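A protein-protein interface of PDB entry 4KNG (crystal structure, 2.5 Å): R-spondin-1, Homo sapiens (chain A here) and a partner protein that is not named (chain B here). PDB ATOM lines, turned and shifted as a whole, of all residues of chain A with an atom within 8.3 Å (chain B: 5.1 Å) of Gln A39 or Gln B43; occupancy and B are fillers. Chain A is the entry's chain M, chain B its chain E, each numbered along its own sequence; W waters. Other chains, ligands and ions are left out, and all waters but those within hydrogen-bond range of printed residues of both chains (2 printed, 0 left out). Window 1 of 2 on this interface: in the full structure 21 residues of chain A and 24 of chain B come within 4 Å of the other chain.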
ATOM      1  N   GLU A  17     -25.760 -20.311 -31.728  1.00  0.00           N
ATOM      2  CA  GLU A  17     -26.009 -19.939 -30.362  1.00  0.00           C
ATOM      3  C   GLU A  17     -24.661 -19.925 -29.656  1.00  0.00           C
ATOM      4  O   GLU A  17     -24.355 -18.990 -28.935  1.00  0.00           O
ATOM      5  CB  GLU A  17     -26.974 -20.909 -29.692  1.00  0.00           C
ATOM      6  CG  GLU A  17     -28.437 -20.528 -29.867  1.00  0.00           C
ATOM      7  CD  GLU A  17     -29.277 -20.927 -28.666  1.00  0.00           C
ATOM      8  OE1 GLU A  17     -29.071 -22.044 -28.127  1.00  0.00           O
ATOM      9  OE2 GLU A  17     -30.136 -20.113 -28.251  1.00  0.00           O
ATOM     10  N   VAL A  18     -23.874 -20.970 -29.883  1.00  0.00           N
ATOM     11  CA  VAL A  18     -22.642 -21.189 -29.145  1.00  0.00           C
ATOM     12  C   VAL A  18     -21.547 -20.222 -29.554  1.00  0.00           C
ATOM     13  O   VAL A  18     -20.926 -19.575 -28.696  1.00  0.00           O
ATOM     14  CB  VAL A  18     -22.141 -22.646 -29.316  1.00  0.00           C
ATOM     15  CG1 VAL A  18     -20.656 -22.762 -29.016  1.00  0.00           C
ATOM     16  CG2 VAL A  18     -22.924 -23.578 -28.403  1.00  0.00           C
ATOM     17  N   ASN A  19     -21.301 -20.165 -30.862  1.00  0.00           N
ATOM     18  CA  ASN A  19     -20.237 -19.332 -31.440  1.00  0.00           C
ATOM     19  C   ASN A  19     -20.656 -17.947 -31.904  1.00  0.00           C
ATOM     20  O   ASN A  19     -19.845 -17.209 -32.386  1.00  0.00           O
ATOM     21  CB  ASN A  19     -19.589 -20.059 -32.584  1.00  0.00           C
ATOM     22  CG  ASN A  19     -18.881 -21.296 -32.141  1.00  0.00           C
ATOM     23  OD1 ASN A  19     -18.926 -22.346 -32.800  1.00  0.00           O
ATOM     24  ND2 ASN A  19     -18.217 -21.197 -31.013  1.00  0.00           N
ATOM     25  N   GLY A  20     -21.903 -17.564 -31.702  1.00  0.00           N
ATOM     26  CA  GLY A  20     -22.375 -16.264 -32.194  1.00  0.00           C
ATOM     27  C   GLY A  20     -22.106 -16.168 -33.677  1.00  0.00           C
ATOM     28  O   GLY A  20     -22.414 -17.088 -34.440  1.00  0.00           O
ATOM     29  N   CYS A  21     -21.479 -15.087 -34.083  1.00  0.00           N
ATOM     30  CA  CYS A  21     -21.267 -14.810 -35.489  1.00  0.00           C
ATOM     31  C   CYS A  21     -20.121 -15.565 -36.149  1.00  0.00           C
ATOM     32  O   CYS A  21     -19.057 -15.751 -35.553  1.00  0.00           O
ATOM     33  CB  CYS A  21     -21.077 -13.323 -35.717  1.00  0.00           C
ATOM     34  SG  CYS A  21     -21.282 -12.995 -37.480  1.00  0.00           S
ATOM     35  N   LEU A  22     -20.346 -15.989 -37.392  1.00  0.00           N
ATOM     36  CA  LEU A  22     -19.342 -16.762 -38.140  1.00  0.00           C
ATOM     37  C   LEU A  22     -18.854 -16.088 -39.428  1.00  0.00           C
ATOM     38  O   LEU A  22     -17.773 -16.398 -39.892  1.00  0.00           O
ATOM     39  CB  LEU A  22     -19.873 -18.166 -38.456  1.00  0.00           C
ATOM     40  CG  LEU A  22     -20.513 -18.912 -37.277  1.00  0.00           C
ATOM     41  CD1 LEU A  22     -21.128 -20.249 -37.709  1.00  0.00           C
ATOM     42  CD2 LEU A  22     -19.464 -19.139 -36.206  1.00  0.00           C
ATOM     43  N   LEU A  31     -14.942  -9.416 -34.550  1.00  0.00           N
ATOM     44  CA  LEU A  31     -14.275  -9.505 -33.270  1.00  0.00           C
ATOM     45  C   LEU A  31     -14.757 -10.736 -32.509  1.00  0.00           C
ATOM     46  O   LEU A  31     -15.962 -10.973 -32.388  1.00  0.00           O
ATOM     47  CB  LEU A  31     -14.569  -8.267 -32.444  1.00  0.00           C
ATOM     48  CG  LEU A  31     -13.940  -8.213 -31.045  1.00  0.00           C
ATOM     49  CD1 LEU A  31     -12.451  -8.548 -31.080  1.00  0.00           C
ATOM     50  CD2 LEU A  31     -14.128  -6.841 -30.427  1.00  0.00           C
ATOM     51  N   LEU A  32     -13.820 -11.516 -32.005  1.00  0.00           N
ATOM     52  CA  LEU A  32     -14.134 -12.581 -31.054  1.00  0.00           C
ATOM     53  C   LEU A  32     -14.160 -12.018 -29.646  1.00  0.00           C
ATOM     54  O   LEU A  32     -13.110 -11.862 -29.059  1.00  0.00           O
ATOM     55  CB  LEU A  32     -13.080 -13.688 -31.167  1.00  0.00           C
ATOM     56  CG  LEU A  32     -12.893 -14.233 -32.574  1.00  0.00           C
ATOM     57  CD1 LEU A  32     -11.973 -15.444 -32.584  1.00  0.00           C
ATOM     58  CD2 LEU A  32     -14.231 -14.640 -33.174  1.00  0.00           C
ATOM     59  N   GLU A  33     -15.346 -11.669 -29.126  1.00  0.00           N
ATOM     60  CA  GLU A  33     -15.530 -11.185 -27.722  1.00  0.00           C
ATOM     61  C   GLU A  33     -15.601 -12.311 -26.680  1.00  0.00           C
ATOM     62  O   GLU A  33     -16.526 -13.149 -26.696  1.00  0.00           O
ATOM     63  CB  GLU A  33     -16.822 -10.406 -27.569  1.00  0.00           C
ATOM     64  CG  GLU A  33     -16.701  -8.900 -27.691  1.00  0.00           C
ATOM     65  CD  GLU A  33     -18.069  -8.234 -27.669  1.00  0.00           C
ATOM     66  OE1 GLU A  33     -19.068  -8.933 -27.351  1.00  0.00           O
ATOM     67  OE2 GLU A  33     -18.163  -7.026 -27.977  1.00  0.00           O
ATOM     68  N   ARG A  34     -14.641 -12.324 -25.760  1.00  0.00           N
ATOM     69  CA  ARG A  34     -14.664 -13.273 -24.641  1.00  0.00           C
ATOM     70  C   ARG A  34     -15.347 -12.724 -23.409  1.00  0.00           C
ATOM     71  O   ARG A  34     -15.081 -11.593 -23.032  1.00  0.00           O
ATOM     72  CB  ARG A  34     -13.253 -13.683 -24.218  1.00  0.00           C
ATOM     73  CG  ARG A  34     -13.287 -14.707 -23.094  1.00  0.00           C
ATOM     74  CD  ARG A  34     -11.975 -15.430 -22.921  1.00  0.00           C
ATOM     75  NE  ARG A  34     -11.752 -16.507 -23.896  1.00  0.00           N
ATOM     76  CZ  ARG A  34     -12.464 -17.626 -23.981  1.00  0.00           C
ATOM     77  NH1 ARG A  34     -13.488 -17.840 -23.172  1.00  0.00           N
ATOM     78  NH2 ARG A  34     -12.163 -18.533 -24.905  1.00  0.00           N
ATOM     79  N   ASN A  35     -16.175 -13.544 -22.758  1.00  0.00           N
ATOM     80  CA  ASN A  35     -16.846 -13.129 -21.528  1.00  0.00           C
ATOM     81  C   ASN A  35     -17.668 -14.211 -20.835  1.00  0.00           C
ATOM     82  O   ASN A  35     -18.769 -14.415 -21.232  1.00  0.00           O
ATOM     83  CB  ASN A  35     -17.818 -11.990 -21.903  1.00  0.00           C
ATOM     84  CG  ASN A  35     -18.863 -11.720 -20.814  1.00  0.00           C
ATOM     85  OD1 ASN A  35     -18.520 -11.497 -19.654  1.00  0.00           O
ATOM     86  ND2 ASN A  35     -20.137 -11.741 -21.187  1.00  0.00           N
ATOM     87  N   ASP A  36     -17.243 -14.928 -19.819  1.00  0.00           N
ATOM     88  CA  ASP A  36     -15.940 -15.178 -19.350  1.00  0.00           C
ATOM     89  C   ASP A  36     -15.600 -16.553 -19.936  1.00  0.00           C
ATOM     90  O   ASP A  36     -14.563 -16.745 -20.524  1.00  0.00           O
ATOM     91  CB  ASP A  36     -16.081 -15.264 -17.803  1.00  0.00           C
ATOM     92  CG  ASP A  36     -14.888 -15.934 -17.097  1.00  0.00           C
ATOM     93  OD1 ASP A  36     -13.712 -15.652 -17.456  1.00  0.00           O
ATOM     94  OD2 ASP A  36     -15.148 -16.737 -16.155  1.00  0.00           O
ATOM     95  N   ILE A  37     -16.483 -17.525 -19.754  1.00  0.00           N
ATOM     96  CA  ILE A  37     -16.307 -18.880 -20.333  1.00  0.00           C
ATOM     97  C   ILE A  37     -16.519 -18.852 -21.860  1.00  0.00           C
ATOM     98  O   ILE A  37     -16.043 -19.718 -22.629  1.00  0.00           O
ATOM     99  CB  ILE A  37     -17.291 -19.875 -19.658  1.00  0.00           C
ATOM    100  CG1 ILE A  37     -16.727 -20.337 -18.330  1.00  0.00           C
ATOM    101  CG2 ILE A  37     -17.591 -21.097 -20.510  1.00  0.00           C
ATOM    102  CD1 ILE A  37     -16.795 -19.296 -17.229  1.00  0.00           C
ATOM    103  N   ARG A  38     -17.246 -17.818 -22.265  1.00  0.00           N
ATOM    104  CA  ARG A  38     -17.752 -17.669 -23.604  1.00  0.00           C
ATOM    105  C   ARG A  38     -16.791 -16.949 -24.508  1.00  0.00           C
ATOM    106  O   ARG A  38     -16.090 -16.045 -24.083  1.00  0.00           O
ATOM    107  CB  ARG A  38     -19.031 -16.860 -23.547  1.00  0.00           C
ATOM    108  CG  ARG A  38     -20.064 -17.495 -22.653  1.00  0.00           C
ATOM    109  CD  ARG A  38     -20.964 -18.427 -23.417  1.00  0.00           C
ATOM    110  NE  ARG A  38     -22.039 -17.606 -23.940  1.00  0.00           N
ATOM    111  CZ  ARG A  38     -22.623 -17.775 -25.117  1.00  0.00           C
ATOM    112  NH1 ARG A  38     -22.258 -18.764 -25.943  1.00  0.00           N
ATOM    113  NH2 ARG A  38     -23.583 -16.922 -25.472  1.00  0.00           N
ATOM    114  N   GLN A  39     -16.779 -17.369 -25.766  1.00  0.00           N
ATOM    115  CA  GLN A  39     -16.107 -16.649 -26.831  1.00  0.00           C
ATOM    116  C   GLN A  39     -17.038 -16.639 -28.036  1.00  0.00           C
ATOM    117  O   GLN A  39     -17.323 -17.689 -28.655  1.00  0.00           O
ATOM    118  CB  GLN A  39     -14.771 -17.287 -27.203  1.00  0.00           C
ATOM    119  CG  GLN A  39     -13.896 -16.351 -28.005  1.00  0.00           C
ATOM    120  CD  GLN A  39     -12.579 -16.950 -28.385  1.00  0.00           C
ATOM    121  OE1 GLN A  39     -12.503 -18.065 -28.925  1.00  0.00           O
ATOM    122  NE2 GLN A  39     -11.504 -16.222 -28.089  1.00  0.00           N
ATOM    123  N   VAL A  40     -17.456 -15.433 -28.396  1.00  0.00           N
ATOM    124  CA  VAL A  40     -18.518 -15.243 -29.340  1.00  0.00           C
ATOM    125  C   VAL A  40     -18.090 -14.274 -30.473  1.00  0.00           C
ATOM    126  O   VAL A  40     -17.287 -13.364 -30.268  1.00  0.00           O
ATOM    127  CB  VAL A  40     -19.750 -14.815 -28.521  1.00  0.00           C
ATOM    128  CG1 VAL A  40     -20.387 -13.528 -29.004  1.00  0.00           C
ATOM    129  CG2 VAL A  40     -20.738 -15.934 -28.521  1.00  0.00           C
ATOM    130  N   GLY A  41     -18.576 -14.529 -31.686  1.00  0.00           N
ATOM    131  CA  GLY A  41     -18.255 -13.709 -32.830  1.00  0.00           C
ATOM    132  C   GLY A  41     -19.170 -12.497 -32.874  1.00  0.00           C
ATOM    133  O   GLY A  41     -20.384 -12.622 -32.771  1.00  0.00           O
ATOM    134  N   VAL A  42     -18.585 -11.318 -33.042  1.00  0.00           N
ATOM    135  CA  VAL A  42     -19.343 -10.072 -33.173  1.00  0.00           C
ATOM    136  C   VAL A  42     -18.834  -9.262 -34.373  1.00  0.00           C
ATOM    137  O   VAL A  42     -17.624  -9.196 -34.639  1.00  0.00           O
ATOM    138  CB  VAL A  42     -19.201  -9.210 -31.901  1.00  0.00           C
ATOM    139  CG1 VAL A  42     -19.878  -7.864 -32.070  1.00  0.00           C
ATOM    140  CG2 VAL A  42     -19.796  -9.926 -30.704  1.00  0.00           C
ATOM    141  N   LEU B  41     -13.248 -25.032 -17.426  1.00  0.00           N
ATOM    142  CA  LEU B  41     -13.850 -25.130 -18.745  1.00  0.00           C
ATOM    143  C   LEU B  41     -13.904 -23.768 -19.405  1.00  0.00           C
ATOM    144  O   LEU B  41     -14.533 -22.836 -18.869  1.00  0.00           O
ATOM    145  CB  LEU B  41     -15.275 -25.667 -18.666  1.00  0.00           C
ATOM    146  CG  LEU B  41     -15.979 -25.858 -20.016  1.00  0.00           C
ATOM    147  CD1 LEU B  41     -15.360 -26.990 -20.836  1.00  0.00           C
ATOM    148  CD2 LEU B  41     -17.464 -26.091 -19.797  1.00  0.00           C
ATOM    149  N   MET B  42     -13.265 -23.682 -20.577  1.00  0.00           N
ATOM    150  CA  MET B  42     -13.311 -22.486 -21.419  1.00  0.00           C
ATOM    151  C   MET B  42     -13.752 -22.816 -22.858  1.00  0.00           C
ATOM    152  O   MET B  42     -13.120 -23.639 -23.557  1.00  0.00           O
ATOM    153  CB  MET B  42     -11.942 -21.796 -21.430  1.00  0.00           C
ATOM    154  CG  MET B  42     -11.493 -21.287 -20.062  1.00  0.00           C
ATOM    155  SD  MET B  42     -12.627 -20.108 -19.277  1.00  0.00           S
ATOM    156  CE  MET B  42     -12.124 -18.551 -20.022  1.00  0.00           C
ATOM    157  N   GLN B  43     -14.836 -22.166 -23.288  1.00  0.00           N
ATOM    158  CA  GLN B  43     -15.260 -22.252 -24.680  1.00  0.00           C
ATOM    159  C   GLN B  43     -14.525 -21.250 -25.545  1.00  0.00           C
ATOM    160  O   GLN B  43     -14.414 -20.088 -25.190  1.00  0.00           O
ATOM    161  CB  GLN B  43     -16.764 -22.020 -24.798  1.00  0.00           C
ATOM    162  CG  GLN B  43     -17.302 -22.075 -26.227  1.00  0.00           C
ATOM    163  CD  GLN B  43     -17.643 -20.702 -26.776  1.00  0.00           C
ATOM    164  OE1 GLN B  43     -18.279 -19.869 -26.111  1.00  0.00           O
ATOM    165  NE2 GLN B  43     -17.247 -20.470 -28.008  1.00  0.00           N
ATOM    166  N   SER B  44     -14.009 -21.715 -26.671  1.00  0.00           N
ATOM    167  CA  SER B  44     -13.402 -20.824 -27.644  1.00  0.00           C
ATOM    168  C   SER B  44     -13.989 -21.040 -29.065  1.00  0.00           C
ATOM    169  O   SER B  44     -14.192 -22.169 -29.503  1.00  0.00           O
ATOM    170  CB  SER B  44     -11.875 -20.953 -27.626  1.00  0.00           C
ATOM    171  OG  SER B  44     -11.462 -22.300 -27.742  1.00  0.00           O
ATOM    172  N   HIS B  45     -14.254 -19.917 -29.741  1.00  0.00           N
ATOM    173  CA  HIS B  45     -14.737 -19.839 -31.122  1.00  0.00           C
ATOM    174  C   HIS B  45     -13.778 -20.553 -32.044  1.00  0.00           C
ATOM    175  O   HIS B  45     -12.573 -20.378 -31.935  1.00  0.00           O
ATOM    176  CB  HIS B  45     -14.797 -18.349 -31.530  1.00  0.00           C
ATOM    177  CG  HIS B  45     -15.760 -18.039 -32.636  1.00  0.00           C
ATOM    178  ND1 HIS B  45     -15.583 -18.487 -33.931  1.00  0.00           N
ATOM    179  CD2 HIS B  45     -16.893 -17.294 -32.643  1.00  0.00           C
ATOM    180  CE1 HIS B  45     -16.586 -18.060 -34.677  1.00  0.00           C
ATOM    181  NE2 HIS B  45     -17.386 -17.321 -33.922  1.00  0.00           N
ATOM    182  N   TYR B  48     -10.824 -18.651 -33.367  1.00  0.00           N
ATOM    183  CA  TYR B  48      -9.744 -18.327 -32.468  1.00  0.00           C
ATOM    184  C   TYR B  48      -8.553 -19.176 -32.807  1.00  0.00           C
ATOM    185  O   TYR B  48      -7.433 -18.680 -32.837  1.00  0.00           O
ATOM    186  CB  TYR B  48     -10.160 -18.515 -31.016  1.00  0.00           C
ATOM    187  CG  TYR B  48      -9.062 -18.314 -29.996  1.00  0.00           C
ATOM    188  CD1 TYR B  48      -8.787 -17.065 -29.485  1.00  0.00           C
ATOM    189  CD2 TYR B  48      -8.338 -19.400 -29.501  1.00  0.00           C
ATOM    190  CE1 TYR B  48      -7.810 -16.888 -28.540  1.00  0.00           C
ATOM    191  CE2 TYR B  48      -7.361 -19.241 -28.546  1.00  0.00           C
ATOM    192  CZ  TYR B  48      -7.098 -17.983 -28.073  1.00  0.00           C
ATOM    193  OH  TYR B  48      -6.109 -17.825 -27.143  1.00  0.00           O
ATOM    194  N   ASP B  56      -5.399 -15.231 -26.153  1.00  0.00           N
ATOM    195  CA  ASP B  56      -6.113 -14.616 -25.038  1.00  0.00           C
ATOM    196  C   ASP B  56      -5.258 -14.610 -23.761  1.00  0.00           C
ATOM    197  O   ASP B  56      -5.565 -13.903 -22.788  1.00  0.00           O
ATOM    198  CB  ASP B  56      -7.423 -15.374 -24.754  1.00  0.00           C
ATOM    199  CG  ASP B  56      -8.616 -14.812 -25.472  1.00  0.00           C
ATOM    200  OD1 ASP B  56      -8.648 -13.582 -25.705  1.00  0.00           O
ATOM    201  OD2 ASP B  56      -9.540 -15.614 -25.750  1.00  0.00           O
ATOM    202  N   ILE B  65     -13.411 -26.106 -24.826  1.00  0.00           N
ATOM    203  CA  ILE B  65     -14.473 -26.718 -25.622  1.00  0.00           C
ATOM    204  C   ILE B  65     -14.676 -25.917 -26.931  1.00  0.00           C
ATOM    205  O   ILE B  65     -14.980 -24.716 -26.910  1.00  0.00           O
ATOM    206  CB  ILE B  65     -15.784 -26.841 -24.817  1.00  0.00           C
ATOM    207  CG1 ILE B  65     -16.919 -27.436 -25.664  1.00  0.00           C
ATOM    208  CG2 ILE B  65     -16.256 -25.510 -24.257  1.00  0.00           C
ATOM    209  CD1 ILE B  65     -16.717 -28.881 -26.062  1.00  0.00           C
ATOM    210  N   VAL B 135     -22.705 -24.526 -20.997  1.00  0.00           N
ATOM    211  CA  VAL B 135     -21.859 -23.391 -21.432  1.00  0.00           C
ATOM    212  C   VAL B 135     -22.639 -22.211 -22.022  1.00  0.00           C
ATOM    213  O   VAL B 135     -22.245 -21.074 -21.862  1.00  0.00           O
ATOM    214  CB  VAL B 135     -20.825 -23.839 -22.477  1.00  0.00           C
ATOM    215  CG1 VAL B 135     -21.469 -23.997 -23.831  1.00  0.00           C
ATOM    216  CG2 VAL B 135     -19.680 -22.850 -22.589  1.00  0.00           C
HETATM  217  O   HOH W   1      -9.888 -18.609 -26.575  1.00  0.00           O
HETATM  218  O   HOH W   2     -16.767 -22.914 -29.619  1.00  0.00           O
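Water W2 lies within hydrogen-bond range of the side-chain amide nitrogen (ND2) of Asn A19 (2.6 Å), the backbone carbonyl oxygen (O) of Ser B44 (2.7 Å) and the side-chain amide nitrogen (NE2) of Gln B43 (3.0 Å).
Water W1 lies within hydrogen-bond range of the guanidinium group of Arg A34, the side-chain carboxylate of Asp B56 and the side-chain amide nitrogen of Gln A39.
Hydrophobic or aromatic side chains of chain A within 4 Å of the printed part of chain B: Leu A22, Leu A32 and Ile A37.
Among the printed residues, Asp or Glu carboxylates within 4 Å of a Lys or Arg side-chain nitrogen of the other chain: Arg A34 with Asp B56 (3.0 Å).
The backbone carbonyl oxygen of Val A18 lies within hydrogen-bond range of the guanidinium group of Arg A38 (3.2 Å).
The backbone NH (N) of Cys A21 sits at hydrogen-bond distance from the backbone carbonyl oxygen (O) of Gly A41 (3.0 Å).
The backbone NH of Glu A33 lies within hydrogen-bond range of the backbone carbonyl oxygen of Val A40.
O of Asp A36 is in hydrogen-bond range of NH1 of Arg A34, at 3.1 Å.
O of Met B42 lies within hydrogen-bond range of N of Ile B65.
The backbone NH (N) of Asp B56 lies within hydrogen-bond range of the side-chain hydroxyl (OH) of Tyr B48, 2.9 Å away.
The side-chain amide nitrogen (ND2) of Asn A19 sits close to the side-chain amide nitrogen (NE2) of Gln B43 (3.2 Å).
A ring nitrogen (NE2) of His B45 is in hydrogen-bond range of the backbone carbonyl oxygen (O) of Asn A19 (2.9 Å).
The backbone carbonyl oxygen (O) of Cys A21 lies within hydrogen-bond range of a ring nitrogen (NE2) of His B45 (2.8 Å).
The backbone carbonyl oxygen of Gln B43 is in hydrogen-bond range of the guanidinium group of Arg A34 (2.8 Å).
The guanidinium group (NE) of Arg A34 is in salt-bridge range of the side-chain carboxylate (OD2) of Asp B56, 3.0 Å away.
The backbone carbonyl oxygen of Ile A37 sits at hydrogen-bond distance from the backbone NH of Gln B43.
The backbone carbonyl oxygen (O) of Gln A39 lies within hydrogen-bond range of the side-chain amide nitrogen (NE2) of Gln B43 (2.9 Å).
The side-chain amide oxygen (OE1) of Gln A39 sits at hydrogen-bond distance from the backbone NH (N) of His B45 (2.7 Å).
The side-chain amide nitrogen of Gln A39 sits at hydrogen-bond distance from the side-chain carboxylate of Asp B56.
Val A18 touches Gln B43.
Leu A22 touches His B45.
Met B42 touches Arg A34.
Arg A34 touches Ser B44.
Met B42 touches Asp A36 (CE to O, 3.1 Å).
Ile A37 touches Leu B41.
CA of Arg A38 touches OE1 of Gln B43, 3.4 Å away.
Ser B44 touches Gln A39 (CA to OE1, 3.2 Å).
Gln A39 touches Tyr B48 (NE2 to CD1, 3.2 Å).
His B45 touches Gly A41.
Gln A39 touches five residues of chain B.
Of the printed residues of chain B, Gly A41 touches His B45.
Of chain A, only Val A18, Asn A19, Arg A34, Ile A37, Arg A38 and Gln A39 come within 4 Å of Gln B43.
Ser B44 touches just these residues of chain A: Arg A34 (3.7 Å) and Gln A39 (3.2 Å).
Of the printed residues of chain A, Val B135 touches Ile A37 (3.4 Å) and Arg A38 (3.3 Å).
The nearest printed residue of chain B that does not touch Gln A39 is Met B42 (6.9 Å).
The nearest printed residue of chain B that does not touch Asn A19 is Ser B44 (4.4 Å).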
